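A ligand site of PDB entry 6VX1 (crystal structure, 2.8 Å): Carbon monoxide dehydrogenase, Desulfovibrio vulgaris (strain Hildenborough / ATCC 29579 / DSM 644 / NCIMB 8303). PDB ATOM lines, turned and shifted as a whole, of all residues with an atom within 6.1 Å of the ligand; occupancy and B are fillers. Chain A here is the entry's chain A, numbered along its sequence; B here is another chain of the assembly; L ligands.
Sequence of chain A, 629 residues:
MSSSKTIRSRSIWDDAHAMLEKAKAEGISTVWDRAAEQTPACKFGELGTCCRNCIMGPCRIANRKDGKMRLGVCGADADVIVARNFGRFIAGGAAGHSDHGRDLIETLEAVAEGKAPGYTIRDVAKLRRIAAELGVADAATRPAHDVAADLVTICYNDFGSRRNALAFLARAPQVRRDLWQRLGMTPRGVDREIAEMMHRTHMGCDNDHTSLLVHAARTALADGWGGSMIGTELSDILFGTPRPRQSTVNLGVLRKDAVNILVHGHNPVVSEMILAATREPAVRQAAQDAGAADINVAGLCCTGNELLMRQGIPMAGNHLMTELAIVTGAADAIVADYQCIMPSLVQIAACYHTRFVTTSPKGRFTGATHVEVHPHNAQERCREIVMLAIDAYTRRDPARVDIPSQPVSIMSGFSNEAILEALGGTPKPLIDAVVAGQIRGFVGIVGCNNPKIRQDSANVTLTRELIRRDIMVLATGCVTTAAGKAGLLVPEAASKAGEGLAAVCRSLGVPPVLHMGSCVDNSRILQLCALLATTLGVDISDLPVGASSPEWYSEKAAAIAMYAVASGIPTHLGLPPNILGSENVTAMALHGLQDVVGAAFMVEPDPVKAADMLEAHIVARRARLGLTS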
ATOM      1  N   HIS A  97       8.252  -1.350  13.275  1.00  0.00           N
ATOM      2  CA  HIS A  97       8.528  -2.242  12.151  1.00  0.00           C
ATOM      3  C   HIS A  97       8.349  -1.540  10.817  1.00  0.00           C
ATOM      4  O   HIS A  97       8.970  -1.936   9.820  1.00  0.00           O
ATOM      5  CB  HIS A  97       7.619  -3.474  12.239  1.00  0.00           C
ATOM      6  CG  HIS A  97       7.763  -4.250  13.504  1.00  0.00           C
ATOM      7  ND1 HIS A  97       6.700  -4.492  14.347  1.00  0.00           N
ATOM      8  CD2 HIS A  97       8.841  -4.829  14.078  1.00  0.00           C
ATOM      9  CE1 HIS A  97       7.115  -5.188  15.387  1.00  0.00           C
ATOM     10  NE2 HIS A  97       8.419  -5.399  15.247  1.00  0.00           N
ATOM     11  N   GLY A 265      20.389  -3.663  18.316  1.00  0.00           N
ATOM     12  CA  GLY A 265      19.306  -3.015  17.605  1.00  0.00           C
ATOM     13  C   GLY A 265      18.552  -4.010  16.724  1.00  0.00           C
ATOM     14  O   GLY A 265      18.360  -5.170  17.110  1.00  0.00           O
ATOM     15  N   HIS A 266      18.130  -3.539  15.558  1.00  0.00           N
ATOM     16  CA  HIS A 266      17.289  -4.312  14.663  1.00  0.00           C
ATOM     17  C   HIS A 266      17.759  -4.352  13.213  1.00  0.00           C
ATOM     18  O   HIS A 266      17.305  -5.237  12.477  1.00  0.00           O
ATOM     19  CB  HIS A 266      15.850  -3.780  14.678  1.00  0.00           C
ATOM     20  CG  HIS A 266      15.131  -4.002  15.970  1.00  0.00           C
ATOM     21  ND1 HIS A 266      15.505  -3.395  17.150  1.00  0.00           N
ATOM     22  CD2 HIS A 266      14.061  -4.779  16.274  1.00  0.00           C
ATOM     23  CE1 HIS A 266      14.704  -3.788  18.117  1.00  0.00           C
ATOM     24  NE2 HIS A 266      13.823  -4.631  17.609  1.00  0.00           N
ATOM     25  N   CYS A 301      20.005  -8.597  20.939  1.00  0.00           N
ATOM     26  CA  CYS A 301      18.627  -8.356  20.532  1.00  0.00           C
ATOM     27  C   CYS A 301      18.391  -8.727  19.062  1.00  0.00           C
ATOM     28  O   CYS A 301      18.956  -9.700  18.574  1.00  0.00           O
ATOM     29  CB  CYS A 301      18.231  -6.904  20.807  1.00  0.00           C
ATOM     30  SG  CYS A 301      17.826  -6.599  22.556  1.00  0.00           S
ATOM     31  N   CYS A 302      17.552  -7.962  18.366  1.00  0.00           N
ATOM     32  CA  CYS A 302      17.048  -8.429  17.073  1.00  0.00           C
ATOM     33  C   CYS A 302      18.117  -8.414  15.988  1.00  0.00           C
ATOM     34  O   CYS A 302      18.144  -9.315  15.140  1.00  0.00           O
ATOM     35  CB  CYS A 302      15.859  -7.585  16.649  1.00  0.00           C
ATOM     36  SG  CYS A 302      14.301  -8.106  17.409  1.00  0.00           S
ATOM     37  N   ASN A 305      19.735 -11.592  16.340  1.00  0.00           N
ATOM     38  CA  ASN A 305      18.957 -12.670  15.725  1.00  0.00           C
ATOM     39  C   ASN A 305      19.167 -12.712  14.216  1.00  0.00           C
ATOM     40  O   ASN A 305      19.259 -13.800  13.630  1.00  0.00           O
ATOM     41  CB  ASN A 305      17.479 -12.507  16.058  1.00  0.00           C
ATOM     42  CG  ASN A 305      17.110 -13.058  17.419  1.00  0.00           C
ATOM     43  OD1 ASN A 305      16.919 -14.262  17.574  1.00  0.00           O
ATOM     44  ND2 ASN A 305      17.021 -12.172  18.410  1.00  0.00           N
ATOM     45  N   ASN A 318      19.812 -11.596  25.443  1.00  0.00           N
ATOM     46  CA  ASN A 318      18.567 -10.927  25.079  1.00  0.00           C
ATOM     47  C   ASN A 318      18.425  -9.589  25.798  1.00  0.00           C
ATOM     48  O   ASN A 318      19.429  -8.928  26.103  1.00  0.00           O
ATOM     49  CB  ASN A 318      17.362 -11.833  25.364  1.00  0.00           C
ATOM     50  CG  ASN A 318      17.515 -12.627  26.643  1.00  0.00           C
ATOM     51  OD1 ASN A 318      18.396 -12.358  27.449  1.00  0.00           O
ATOM     52  ND2 ASN A 318      16.653 -13.624  26.821  1.00  0.00           N
ATOM     53  N   HIS A 319      17.182  -9.186  26.079  1.00  0.00           N
ATOM     54  CA  HIS A 319      16.885  -7.806  26.452  1.00  0.00           C
ATOM     55  C   HIS A 319      17.606  -7.383  27.734  1.00  0.00           C
ATOM     56  O   HIS A 319      18.400  -6.443  27.736  1.00  0.00           O
ATOM     57  CB  HIS A 319      15.374  -7.628  26.614  1.00  0.00           C
ATOM     58  CG  HIS A 319      14.974  -6.273  27.112  1.00  0.00           C
ATOM     59  ND1 HIS A 319      15.580  -5.107  26.679  1.00  0.00           N
ATOM     60  CD2 HIS A 319      14.041  -5.894  28.022  1.00  0.00           C
ATOM     61  CE1 HIS A 319      15.035  -4.071  27.295  1.00  0.00           C
ATOM     62  NE2 HIS A 319      14.097  -4.525  28.115  1.00  0.00           N
ATOM     63  N   GLN A 339      15.775   1.180  18.048  1.00  0.00           N
ATOM     64  CA  GLN A 339      14.742   0.353  18.667  1.00  0.00           C
ATOM     65  C   GLN A 339      15.263  -0.539  19.795  1.00  0.00           C
ATOM     66  O   GLN A 339      16.204  -1.327  19.594  1.00  0.00           O
ATOM     67  CB  GLN A 339      14.033  -0.521  17.629  1.00  0.00           C
ATOM     68  CG  GLN A 339      13.066   0.225  16.749  1.00  0.00           C
ATOM     69  CD  GLN A 339      12.614  -0.628  15.578  1.00  0.00           C
ATOM     70  OE1 GLN A 339      12.091  -0.122  14.594  1.00  0.00           O
ATOM     71  NE2 GLN A 339      12.841  -1.935  15.682  1.00  0.00           N
ATOM     72  N   CYS A 340      14.661  -0.411  20.977  1.00  0.00           N
ATOM     73  CA  CYS A 340      14.905  -1.267  22.138  1.00  0.00           C
ATOM     74  C   CYS A 340      16.348  -1.215  22.620  1.00  0.00           C
ATOM     75  O   CYS A 340      16.825  -2.165  23.267  1.00  0.00           O
ATOM     76  CB  CYS A 340      14.492  -2.723  21.840  1.00  0.00           C
ATOM     77  SG  CYS A 340      12.702  -2.971  21.653  1.00  0.00           S
ATOM     78  N   VAL A 446       7.111 -15.328  21.131  1.00  0.00           N
ATOM     79  CA  VAL A 446       7.675 -14.155  20.474  1.00  0.00           C
ATOM     80  C   VAL A 446       8.012 -13.066  21.492  1.00  0.00           C
ATOM     81  O   VAL A 446       8.258 -11.905  21.106  1.00  0.00           O
ATOM     82  CB  VAL A 446       6.695 -13.620  19.418  1.00  0.00           C
ATOM     83  CG1 VAL A 446       6.290 -14.745  18.463  1.00  0.00           C
ATOM     84  CG2 VAL A 446       5.454 -13.039  20.082  1.00  0.00           C
ATOM     85  N   GLY A 447       8.047 -13.416  22.767  1.00  0.00           N
ATOM     86  CA  GLY A 447       8.147 -12.446  23.833  1.00  0.00           C
ATOM     87  C   GLY A 447       9.495 -11.762  23.969  1.00  0.00           C
ATOM     88  O   GLY A 447      10.471 -12.055  23.271  1.00  0.00           O
ATOM     89  N   CYS A 448       9.540 -10.810  24.910  1.00  0.00           N
ATOM     90  CA  CYS A 448      10.770 -10.125  25.283  1.00  0.00           C
ATOM     91  C   CYS A 448      11.237 -10.557  26.671  1.00  0.00           C
ATOM     92  O   CYS A 448      11.126 -11.734  27.032  1.00  0.00           O
ATOM     93  CB  CYS A 448      10.566  -8.602  25.297  1.00  0.00           C
ATOM     94  SG  CYS A 448       9.435  -7.905  24.064  1.00  0.00           S
ATOM     95  N   ASN A 449      11.764  -9.599  27.427  1.00  0.00           N
ATOM     96  CA  ASN A 449      11.974  -9.735  28.857  1.00  0.00           C
ATOM     97  C   ASN A 449      11.288  -8.559  29.552  1.00  0.00           C
ATOM     98  O   ASN A 449      11.077  -7.516  28.939  1.00  0.00           O
ATOM     99  CB  ASN A 449      13.465  -9.753  29.226  1.00  0.00           C
ATOM    100  CG  ASN A 449      14.128 -11.080  28.903  1.00  0.00           C
ATOM    101  OD1 ASN A 449      13.516 -12.146  29.019  1.00  0.00           O
ATOM    102  ND2 ASN A 449      15.389 -11.023  28.511  1.00  0.00           N
ATOM    103  N   THR A 476      11.054 -16.694  18.187  1.00  0.00           N
ATOM    104  CA  THR A 476      11.607 -15.475  17.623  1.00  0.00           C
ATOM    105  C   THR A 476      11.937 -14.509  18.748  1.00  0.00           C
ATOM    106  O   THR A 476      11.420 -14.617  19.863  1.00  0.00           O
ATOM    107  CB  THR A 476      10.650 -14.786  16.637  1.00  0.00           C
ATOM    108  OG1 THR A 476       9.483 -14.335  17.329  1.00  0.00           O
ATOM    109  CG2 THR A 476      10.247 -15.717  15.505  1.00  0.00           C
ATOM    110  N   GLY A 477      12.824 -13.555  18.451  1.00  0.00           N
ATOM    111  CA  GLY A 477      13.110 -12.483  19.398  1.00  0.00           C
ATOM    112  C   GLY A 477      13.907 -12.956  20.597  1.00  0.00           C
ATOM    113  O   GLY A 477      14.876 -13.713  20.480  1.00  0.00           O
ATOM    114  N   CYS A 478      13.493 -12.485  21.781  1.00  0.00           N
ATOM    115  CA  CYS A 478      14.230 -12.752  23.009  1.00  0.00           C
ATOM    116  C   CYS A 478      14.203 -14.220  23.389  1.00  0.00           C
ATOM    117  O   CYS A 478      15.172 -14.728  23.970  1.00  0.00           O
ATOM    118  CB  CYS A 478      13.656 -11.918  24.165  1.00  0.00           C
ATOM    119  SG  CYS A 478      14.250 -10.216  24.258  1.00  0.00           S
ATOM    120  N   VAL A 479      13.114 -14.922  23.077  1.00  0.00           N
ATOM    121  CA  VAL A 479      12.987 -16.338  23.432  1.00  0.00           C
ATOM    122  C   VAL A 479      14.104 -17.170  22.817  1.00  0.00           C
ATOM    123  O   VAL A 479      14.417 -18.258  23.334  1.00  0.00           O
ATOM    124  CB  VAL A 479      11.602 -16.855  22.986  1.00  0.00           C
ATOM    125  CG1 VAL A 479      11.311 -18.217  23.598  1.00  0.00           C
ATOM    126  CG2 VAL A 479      10.535 -15.848  23.389  1.00  0.00           C
ATOM    127  N   SER A 518      14.086 -12.750  13.999  1.00  0.00           N
ATOM    128  CA  SER A 518      13.939 -11.570  14.850  1.00  0.00           C
ATOM    129  C   SER A 518      12.464 -11.236  15.033  1.00  0.00           C
ATOM    130  O   SER A 518      11.578 -12.044  14.735  1.00  0.00           O
ATOM    131  CB  SER A 518      14.740 -10.416  14.258  1.00  0.00           C
ATOM    132  OG  SER A 518      14.399 -10.217  12.896  1.00  0.00           O
ATOM    133  N   CYS A 519      12.181 -10.028  15.515  1.00  0.00           N
ATOM    134  CA  CYS A 519      10.795  -9.618  15.745  1.00  0.00           C
ATOM    135  C   CYS A 519      10.042  -9.439  14.427  1.00  0.00           C
ATOM    136  O   CYS A 519       8.869  -9.807  14.325  1.00  0.00           O
ATOM    137  CB  CYS A 519      10.751  -8.339  16.566  1.00  0.00           C
ATOM    138  SG  CYS A 519      10.487  -8.600  18.337  1.00  0.00           S
ATOM    139  N   VAL A 520      10.697  -8.870  13.417  1.00  0.00           N
ATOM    140  CA  VAL A 520      10.051  -8.747  12.119  1.00  0.00           C
ATOM    141  C   VAL A 520       9.862 -10.109  11.474  1.00  0.00           C
ATOM    142  O   VAL A 520       8.953 -10.289  10.656  1.00  0.00           O
ATOM    143  CB  VAL A 520      10.830  -7.792  11.180  1.00  0.00           C
ATOM    144  CG1 VAL A 520      11.002  -6.454  11.848  1.00  0.00           C
ATOM    145  CG2 VAL A 520      12.167  -8.377  10.786  1.00  0.00           C
ATOM    146  N   TYR A 553       7.141  -6.461  26.837  1.00  0.00           N
ATOM    147  CA  TYR A 553       7.106  -5.113  27.404  1.00  0.00           C
ATOM    148  C   TYR A 553       6.801  -4.011  26.391  1.00  0.00           C
ATOM    149  O   TYR A 553       6.228  -2.988  26.783  1.00  0.00           O
ATOM    150  CB  TYR A 553       8.428  -4.773  28.113  1.00  0.00           C
ATOM    151  CG  TYR A 553       9.532  -4.407  27.149  1.00  0.00           C
ATOM    152  CD1 TYR A 553       9.752  -3.086  26.788  1.00  0.00           C
ATOM    153  CD2 TYR A 553      10.354  -5.381  26.600  1.00  0.00           C
ATOM    154  CE1 TYR A 553      10.740  -2.739  25.901  1.00  0.00           C
ATOM    155  CE2 TYR A 553      11.353  -5.040  25.717  1.00  0.00           C
ATOM    156  CZ  TYR A 553      11.547  -3.726  25.365  1.00  0.00           C
ATOM    157  OH  TYR A 553      12.547  -3.386  24.482  1.00  0.00           O
ATOM    158  N   SER A 554       7.161  -4.165  25.114  1.00  0.00           N
ATOM    159  CA  SER A 554       7.233  -3.052  24.192  1.00  0.00           C
ATOM    160  C   SER A 554       5.935  -2.851  23.411  1.00  0.00           C
ATOM    161  O   SER A 554       5.014  -3.673  23.444  1.00  0.00           O
ATOM    162  CB  SER A 554       8.385  -3.241  23.213  1.00  0.00           C
ATOM    163  OG  SER A 554       8.129  -4.329  22.339  1.00  0.00           O
ATOM    164  N   LYS A 556       6.050  -2.793  20.151  1.00  0.00           N
ATOM    165  CA  LYS A 556       6.180  -3.697  19.017  1.00  0.00           C
ATOM    166  C   LYS A 556       5.657  -5.087  19.343  1.00  0.00           C
ATOM    167  O   LYS A 556       5.112  -5.764  18.460  1.00  0.00           O
ATOM    168  CB  LYS A 556       7.641  -3.770  18.547  1.00  0.00           C
ATOM    169  CG  LYS A 556       8.226  -2.410  18.178  1.00  0.00           C
ATOM    170  CD  LYS A 556       9.455  -2.492  17.259  1.00  0.00           C
ATOM    171  CE  LYS A 556      10.667  -3.081  17.965  1.00  0.00           C
ATOM    172  NZ  LYS A 556      10.724  -4.572  17.841  1.00  0.00           N
ATOM    173  N   ALA A 557       5.807  -5.523  20.595  1.00  0.00           N
ATOM    174  CA  ALA A 557       5.265  -6.814  20.983  1.00  0.00           C
ATOM    175  C   ALA A 557       3.750  -6.817  20.951  1.00  0.00           C
ATOM    176  O   ALA A 557       3.136  -7.804  20.522  1.00  0.00           O
ATOM    177  CB  ALA A 557       5.768  -7.199  22.379  1.00  0.00           C
ATOM    178  N   ILE A 560       2.557  -7.047  17.420  1.00  0.00           N
ATOM    179  CA  ILE A 560       2.702  -8.426  16.966  1.00  0.00           C
ATOM    180  C   ILE A 560       1.568  -9.273  17.522  1.00  0.00           C
ATOM    181  O   ILE A 560       0.935 -10.055  16.795  1.00  0.00           O
ATOM    182  CB  ILE A 560       4.078  -8.987  17.368  1.00  0.00           C
ATOM    183  CG1 ILE A 560       5.191  -8.326  16.545  1.00  0.00           C
ATOM    184  CG2 ILE A 560       4.114 -10.489  17.218  1.00  0.00           C
ATOM    185  CD1 ILE A 560       6.585  -8.536  17.109  1.00  0.00           C
ATOM    186  N   HIS B 202       9.286   5.488  20.280  1.00  0.00           N
ATOM    187  CA  HIS B 202       9.292   4.148  20.853  1.00  0.00           C
ATOM    188  C   HIS B 202      10.487   3.994  21.798  1.00  0.00           C
ATOM    189  O   HIS B 202      11.491   4.701  21.693  1.00  0.00           O
ATOM    190  CB  HIS B 202       9.356   3.108  19.737  1.00  0.00           C
ATOM    191  CG  HIS B 202       9.247   1.684  20.205  1.00  0.00           C
ATOM    192  ND1 HIS B 202       8.045   1.033  20.337  1.00  0.00           N
ATOM    193  CD2 HIS B 202      10.203   0.797  20.571  1.00  0.00           C
ATOM    194  CE1 HIS B 202       8.259  -0.196  20.773  1.00  0.00           C
ATOM    195  NE2 HIS B 202       9.560  -0.372  20.918  1.00  0.00           N
HETATM  196 NI1  LIG L   1      12.958  -6.412  18.139  1.00  0.00          NI
HETATM  197  S1  LIG L   1      11.563  -9.761  21.408  1.00  0.00           S
HETATM  198  S2  LIG L   1      13.030  -6.614  23.222  1.00  0.00           S
HETATM  199  S3  LIG L   1      15.073  -9.372  20.746  1.00  0.00           S
HETATM  200  S4  LIG L   1      10.008  -5.930  20.804  1.00  0.00           S
HETATM  201 FE1  LIG L   1      12.356  -5.209  21.335  1.00  0.00          FE
HETATM  202 FE2  LIG L   1      14.083  -7.142  20.084  1.00  0.00          FE
HETATM  203 FE3  LIG L   1      10.878  -7.568  22.325  1.00  0.00          FE
HETATM  204 FE4  LIG L   1      13.542  -8.915  22.527  1.00  0.00          FE
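NE2 of His 266 is bound to NI1 of the ligand (2.0 Å).
A sulfur (S1) of the ligand sits close to the backbone NH of Cys 478 (3.4 Å).
The side-chain sulfur of Cys 478 binds an iron atom (FE4) of the ligand.
S3 of the ligand lies close to N of Cys 302 (3.7 Å).
NI1 of the ligand is bound by SG of Cys 302.
SG of Cys 448 is bound to FE3 of the ligand, 2.3 Å away.
SG of Cys 340 binds FE1 of the ligand, 2.3 Å away.
The side-chain hydroxyl (OG) of Ser 554 sits close to a sulfur (S4) of the ligand, at 2.9 Å.
The side-chain amino group of Lys 556 lies close to a sulfur (S4) of the ligand, at 3.3 Å.
SG of Cys 519 lies close to S1 of the ligand, 3.5 Å away.
OH of Tyr 553 lies close to S2 of the ligand (3.5 Å).
A ring nitrogen (ND1) of His 266 sits close to the backbone carbonyl oxygen (O) of Gln 339, 3.3 Å away.
The side-chain sulfur (SG) of Cys 478 lies close to the backbone NH (N) of His 319, 3.6 Å away.
N of Cys 302 sits at hydrogen-bond distance from O of Gly 265 (3.2 Å).
SG of Cys 340 sits close to OH of Tyr 553 (2.9 Å).
The side-chain hydroxyl of Ser 554 sits close to the backbone NH of Lys 556, 3.4 Å away.
N of Ala 557 lies within hydrogen-bond range of OG of Ser 554 (3.1 Å).
The backbone carbonyl oxygen (O) of Cys 301 is in hydrogen-bond range of the side-chain amide nitrogen (ND2) of Asn 305 (3.1 Å).
The backbone carbonyl oxygen (O) of Gly 477 is in hydrogen-bond range of the side-chain amide nitrogen (ND2) of Asn 305.
S1 of the ligand lies close to O of Gly 447, 3.2 Å away.
Cys 301 touches the ligand (CA to S3, 3.7 Å).
O of Val 446 touches S1 of the ligand, 3.95 Å away.
Gly 477 touches the ligand (CA to S1, 3.7 Å).
Hydrophobic or aromatic side chains that line the ligand: His 266 and Tyr 553.
Of the 27 residues printed, 13 come within 4 Å of the ligand.
The nearest printed residue that does not touch the ligand is Asn 305 (4.1 Å).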
